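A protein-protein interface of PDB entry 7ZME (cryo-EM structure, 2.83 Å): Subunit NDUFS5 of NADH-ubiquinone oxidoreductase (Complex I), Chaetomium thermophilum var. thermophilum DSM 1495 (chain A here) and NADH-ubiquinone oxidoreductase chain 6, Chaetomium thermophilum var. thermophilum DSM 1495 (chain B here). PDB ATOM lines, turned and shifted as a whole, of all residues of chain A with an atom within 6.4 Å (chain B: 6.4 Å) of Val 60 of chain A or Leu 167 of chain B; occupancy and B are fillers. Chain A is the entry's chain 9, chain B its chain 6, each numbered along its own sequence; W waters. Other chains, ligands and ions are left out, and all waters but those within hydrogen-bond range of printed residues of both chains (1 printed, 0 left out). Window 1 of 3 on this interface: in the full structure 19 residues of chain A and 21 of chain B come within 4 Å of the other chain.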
ATOM      1  N   LYS A  55      -2.530  -8.739 -26.071  1.00  0.00           N
ATOM      2  CA  LYS A  55      -3.569  -9.712 -26.489  1.00  0.00           C
ATOM      3  C   LYS A  55      -3.140 -11.117 -26.068  1.00  0.00           C
ATOM      4  O   LYS A  55      -4.023 -11.923 -25.774  1.00  0.00           O
ATOM      5  CB  LYS A  55      -3.861  -9.631 -27.991  1.00  0.00           C
ATOM      6  CG  LYS A  55      -4.204  -8.256 -28.537  1.00  0.00           C
ATOM      7  CD  LYS A  55      -4.342  -8.253 -30.037  1.00  0.00           C
ATOM      8  CE  LYS A  55      -5.427  -9.193 -30.514  1.00  0.00           C
ATOM      9  NZ  LYS A  55      -5.443  -9.312 -31.991  1.00  0.00           N
ATOM     10  N   GLU A  56      -1.839 -11.400 -26.058  1.00  0.00           N
ATOM     11  CA  GLU A  56      -1.378 -12.773 -25.728  1.00  0.00           C
ATOM     12  C   GLU A  56      -1.365 -12.924 -24.217  1.00  0.00           C
ATOM     13  O   GLU A  56      -1.528 -14.052 -23.725  1.00  0.00           O
ATOM     14  CB  GLU A  56       0.038 -13.024 -26.233  1.00  0.00           C
ATOM     15  CG  GLU A  56       0.532 -14.439 -26.009  1.00  0.00           C
ATOM     16  CD  GLU A  56       2.043 -14.602 -26.000  1.00  0.00           C
ATOM     17  OE1 GLU A  56       2.742 -13.681 -26.465  1.00  0.00           O
ATOM     18  OE2 GLU A  56       2.517 -15.649 -25.523  1.00  0.00           O
ATOM     19  N   ALA A  57      -1.201 -11.806 -23.513  1.00  0.00           N
ATOM     20  CA  ALA A  57      -1.151 -11.892 -22.044  1.00  0.00           C
ATOM     21  C   ALA A  57      -2.581 -12.086 -21.570  1.00  0.00           C
ATOM     22  O   ALA A  57      -2.792 -12.750 -20.546  1.00  0.00           O
ATOM     23  CB  ALA A  57      -0.579 -10.613 -21.496  1.00  0.00           C
ATOM     24  N   ALA A  58      -3.522 -11.531 -22.327  1.00  0.00           N
ATOM     25  CA  ALA A  58      -4.925 -11.722 -21.985  1.00  0.00           C
ATOM     26  C   ALA A  58      -5.383 -13.138 -22.301  1.00  0.00           C
ATOM     27  O   ALA A  58      -6.207 -13.704 -21.577  1.00  0.00           O
ATOM     28  CB  ALA A  58      -5.785 -10.699 -22.718  1.00  0.00           C
ATOM     29  N   ARG A  59      -4.865 -13.726 -23.378  1.00  0.00           N
ATOM     30  CA  ARG A  59      -5.233 -15.097 -23.714  1.00  0.00           C
ATOM     31  C   ARG A  59      -4.703 -16.078 -22.680  1.00  0.00           C
ATOM     32  O   ARG A  59      -5.446 -16.929 -22.179  1.00  0.00           O
ATOM     33  CB  ARG A  59      -4.715 -15.464 -25.099  1.00  0.00           C
ATOM     34  CG  ARG A  59      -5.255 -16.787 -25.592  1.00  0.00           C
ATOM     35  CD  ARG A  59      -4.341 -17.405 -26.627  1.00  0.00           C
ATOM     36  NE  ARG A  59      -3.133 -17.943 -26.016  1.00  0.00           N
ATOM     37  CZ  ARG A  59      -2.862 -19.237 -25.910  1.00  0.00           C
ATOM     38  NH1 ARG A  59      -3.710 -20.134 -26.387  1.00  0.00           N
ATOM     39  NH2 ARG A  59      -1.735 -19.634 -25.339  1.00  0.00           N
ATOM     40  N   VAL A  60      -3.413 -15.982 -22.355  1.00  0.00           N
ATOM     41  CA  VAL A  60      -2.821 -16.894 -21.383  1.00  0.00           C
ATOM     42  C   VAL A  60      -3.468 -16.707 -20.021  1.00  0.00           C
ATOM     43  O   VAL A  60      -3.717 -17.677 -19.299  1.00  0.00           O
ATOM     44  CB  VAL A  60      -1.293 -16.696 -21.330  1.00  0.00           C
ATOM     45  CG1 VAL A  60      -0.706 -17.347 -20.096  1.00  0.00           C
ATOM     46  CG2 VAL A  60      -0.647 -17.261 -22.583  1.00  0.00           C
ATOM     47  N   ARG A  61      -3.778 -15.460 -19.657  1.00  0.00           N
ATOM     48  CA  ARG A  61      -4.409 -15.191 -18.369  1.00  0.00           C
ATOM     49  C   ARG A  61      -5.740 -15.921 -18.240  1.00  0.00           C
ATOM     50  O   ARG A  61      -5.995 -16.595 -17.236  1.00  0.00           O
ATOM     51  CB  ARG A  61      -4.604 -13.686 -18.186  1.00  0.00           C
ATOM     52  CG  ARG A  61      -4.412 -13.208 -16.762  1.00  0.00           C
ATOM     53  CD  ARG A  61      -4.596 -11.704 -16.649  1.00  0.00           C
ATOM     54  NE  ARG A  61      -3.749 -10.967 -17.581  1.00  0.00           N
ATOM     55  CZ  ARG A  61      -2.507 -10.578 -17.314  1.00  0.00           C
ATOM     56  NH1 ARG A  61      -1.960 -10.858 -16.140  1.00  0.00           N
ATOM     57  NH2 ARG A  61      -1.810  -9.912 -18.221  1.00  0.00           N
ATOM     58  N   ALA A  62      -6.605 -15.792 -19.247  1.00  0.00           N
ATOM     59  CA  ALA A  62      -7.874 -16.516 -19.231  1.00  0.00           C
ATOM     60  C   ALA A  62      -7.655 -18.021 -19.272  1.00  0.00           C
ATOM     61  O   ALA A  62      -8.322 -18.771 -18.551  1.00  0.00           O
ATOM     62  CB  ALA A  62      -8.744 -16.072 -20.404  1.00  0.00           C
ATOM     63  N   LEU A  63      -6.727 -18.481 -20.108  1.00  0.00           N
ATOM     64  CA  LEU A  63      -6.460 -19.909 -20.216  1.00  0.00           C
ATOM     65  C   LEU A  63      -5.812 -20.466 -18.954  1.00  0.00           C
ATOM     66  O   LEU A  63      -6.048 -21.624 -18.602  1.00  0.00           O
ATOM     67  CB  LEU A  63      -5.576 -20.175 -21.435  1.00  0.00           C
ATOM     68  CG  LEU A  63      -5.435 -21.611 -21.941  1.00  0.00           C
ATOM     69  CD1 LEU A  63      -6.781 -22.303 -22.007  1.00  0.00           C
ATOM     70  CD2 LEU A  63      -4.753 -21.625 -23.298  1.00  0.00           C
ATOM     71  N   GLN A  64      -4.999 -19.666 -18.262  1.00  0.00           N
ATOM     72  CA  GLN A  64      -4.299 -20.172 -17.087  1.00  0.00           C
ATOM     73  C   GLN A  64      -5.215 -20.281 -15.875  1.00  0.00           C
ATOM     74  O   GLN A  64      -5.073 -21.216 -15.081  1.00  0.00           O
ATOM     75  CB  GLN A  64      -3.101 -19.280 -16.765  1.00  0.00           C
ATOM     76  CG  GLN A  64      -2.243 -19.765 -15.620  1.00  0.00           C
ATOM     77  CD  GLN A  64      -1.053 -18.875 -15.395  1.00  0.00           C
ATOM     78  OE1 GLN A  64      -0.888 -17.867 -16.076  1.00  0.00           O
ATOM     79  NE2 GLN A  64      -0.194 -19.256 -14.465  1.00  0.00           N
ATOM     80  N   ALA A  65      -6.142 -19.340 -15.705  1.00  0.00           N
ATOM     81  CA  ALA A  65      -7.116 -19.468 -14.629  1.00  0.00           C
ATOM     82  C   ALA A  65      -8.088 -20.603 -14.912  1.00  0.00           C
ATOM     83  O   ALA A  65      -8.482 -21.336 -13.998  1.00  0.00           O
ATOM     84  CB  ALA A  65      -7.863 -18.151 -14.434  1.00  0.00           C
ATOM     85  N   TYR B 127       3.009  -1.859 -22.210  1.00  0.00           N
ATOM     86  CA  TYR B 127       2.730  -3.057 -21.370  1.00  0.00           C
ATOM     87  C   TYR B 127       4.025  -3.719 -20.906  1.00  0.00           C
ATOM     88  O   TYR B 127       4.073  -4.176 -19.759  1.00  0.00           O
ATOM     89  CB  TYR B 127       1.891  -4.046 -22.171  1.00  0.00           C
ATOM     90  CG  TYR B 127       0.984  -4.938 -21.369  1.00  0.00           C
ATOM     91  CD1 TYR B 127       0.026  -4.404 -20.528  1.00  0.00           C
ATOM     92  CD2 TYR B 127       1.060  -6.315 -21.479  1.00  0.00           C
ATOM     93  CE1 TYR B 127      -0.823  -5.214 -19.795  1.00  0.00           C
ATOM     94  CE2 TYR B 127       0.218  -7.140 -20.756  1.00  0.00           C
ATOM     95  CZ  TYR B 127      -0.725  -6.588 -19.910  1.00  0.00           C
ATOM     96  OH  TYR B 127      -1.560  -7.389 -19.189  1.00  0.00           O
ATOM     97  N   ASN B 165      -3.217 -15.087  -9.638  1.00  0.00           N
ATOM     98  CA  ASN B 165      -2.920 -15.828 -10.863  1.00  0.00           C
ATOM     99  C   ASN B 165      -2.125 -14.909 -11.783  1.00  0.00           C
ATOM    100  O   ASN B 165      -2.704 -14.152 -12.567  1.00  0.00           O
ATOM    101  CB  ASN B 165      -4.196 -16.328 -11.543  1.00  0.00           C
ATOM    102  N   ASP B 166      -0.802 -14.978 -11.687  1.00  0.00           N
ATOM    103  CA  ASP B 166       0.092 -14.132 -12.461  1.00  0.00           C
ATOM    104  C   ASP B 166       0.607 -14.884 -13.682  1.00  0.00           C
ATOM    105  O   ASP B 166       0.416 -16.092 -13.829  1.00  0.00           O
ATOM    106  CB  ASP B 166       1.264 -13.648 -11.598  1.00  0.00           C
ATOM    107  CG  ASP B 166       0.807 -12.879 -10.376  1.00  0.00           C
ATOM    108  OD1 ASP B 166      -0.333 -12.369 -10.384  1.00  0.00           O
ATOM    109  OD2 ASP B 166       1.588 -12.783  -9.406  1.00  0.00           O
ATOM    110  N   LEU B 167       1.269 -14.145 -14.561  1.00  0.00           N
ATOM    111  CA  LEU B 167       1.794 -14.705 -15.795  1.00  0.00           C
ATOM    112  C   LEU B 167       3.272 -15.027 -15.651  1.00  0.00           C
ATOM    113  O   LEU B 167       3.969 -14.504 -14.782  1.00  0.00           O
ATOM    114  CB  LEU B 167       1.583 -13.743 -16.961  1.00  0.00           C
ATOM    115  CG  LEU B 167       0.132 -13.474 -17.354  1.00  0.00           C
ATOM    116  CD1 LEU B 167       0.088 -12.821 -18.710  1.00  0.00           C
ATOM    117  CD2 LEU B 167      -0.695 -14.754 -17.338  1.00  0.00           C
ATOM    118  N   PHE B 168       3.737 -15.944 -16.491  1.00  0.00           N
ATOM    119  CA  PHE B 168       5.159 -16.359 -16.463  1.00  0.00           C
ATOM    120  C   PHE B 168       5.722 -16.265 -17.876  1.00  0.00           C
ATOM    121  O   PHE B 168       5.086 -16.754 -18.823  1.00  0.00           O
ATOM    122  CB  PHE B 168       5.310 -17.769 -15.895  1.00  0.00           C
ATOM    123  CG  PHE B 168       5.059 -17.850 -14.412  1.00  0.00           C
ATOM    124  CD1 PHE B 168       6.071 -17.575 -13.508  1.00  0.00           C
ATOM    125  CD2 PHE B 168       3.807 -18.176 -13.920  1.00  0.00           C
ATOM    126  CE1 PHE B 168       5.838 -17.634 -12.145  1.00  0.00           C
ATOM    127  CE2 PHE B 168       3.575 -18.237 -12.556  1.00  0.00           C
ATOM    128  CZ  PHE B 168       4.592 -17.967 -11.670  1.00  0.00           C
ATOM    129  N   PHE B 169       6.865 -15.597 -18.003  1.00  0.00           N
ATOM    130  CA  PHE B 169       7.537 -15.482 -19.316  1.00  0.00           C
ATOM    131  C   PHE B 169       8.178 -16.816 -19.673  1.00  0.00           C
ATOM    132  O   PHE B 169       8.784 -17.446 -18.808  1.00  0.00           O
ATOM    133  CB  PHE B 169       8.516 -14.312 -19.294  1.00  0.00           C
ATOM    134  CG  PHE B 169       7.872 -12.962 -19.125  1.00  0.00           C
ATOM    135  CD1 PHE B 169       7.197 -12.366 -20.174  1.00  0.00           C
ATOM    136  CD2 PHE B 169       7.942 -12.290 -17.919  1.00  0.00           C
ATOM    137  CE1 PHE B 169       6.609 -11.122 -20.017  1.00  0.00           C
ATOM    138  CE2 PHE B 169       7.349 -11.048 -17.763  1.00  0.00           C
ATOM    139  CZ  PHE B 169       6.682 -10.467 -18.813  1.00  0.00           C
HETATM  140  O   HOH W   1       1.878 -18.183 -16.669  1.00  0.00           O
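Of the 11 printed residues of chain A, 4 touch a printed residue of chain B. Among the printed residues, 7 pairs touch across the chains.
Of the printed residues of chain B, Val 60 of chain A touches Leu 167. Of the printed residues of chain A, Leu 167 of chain B touches Ala 57, Val 60, Arg 61 and Gln 64. Of the printed residues of chain B, Arg 61 of chain A touches Tyr 127 and Leu 167. Printed residues of chain B within 4 Å of Gln 64 of chain A: Asp 166 and Leu 167. Printed residues of chain A within 4 Å of Asp 166 of chain B: Gln 64. The nearest residue of chain B that does not touch Val 60 of chain A is Phe 168 of chain B (5.9 Å). The nearest printed residue of chain A that does not touch Asp 166 of chain B is Arg 61 of chain A (5.3 Å).
The side-chain amide oxygen (OE1) of Gln 64 of chain A lies close to the backbone carbonyl oxygen (O) of Asp 166 of chain B (3.1 Å). OH of Tyr 127 of chain B is in hydrogen-bond range of NH2 of Arg 61 of chain A, at 2.7 Å.
Water W1 lies within hydrogen-bond range of the side-chain amide oxygen (OE1) of Gln 64 of chain A and the backbone NH (N) of Phe 168 of chain B.
CE2 of Tyr 127 of chain B touches CB of Ala 57 of chain A (3.6 Å). Ala 57 of chain A touches Leu 167 of chain B. CD2 of Leu 167 of chain B touches CG1 of Val 60 of chain A, 3.8 Å away. Leu 167 of chain B touches Arg 61 of chain A (CD1 to NH2, 3.5 Å). Gln 64 of chain A touches Leu 167 of chain B.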
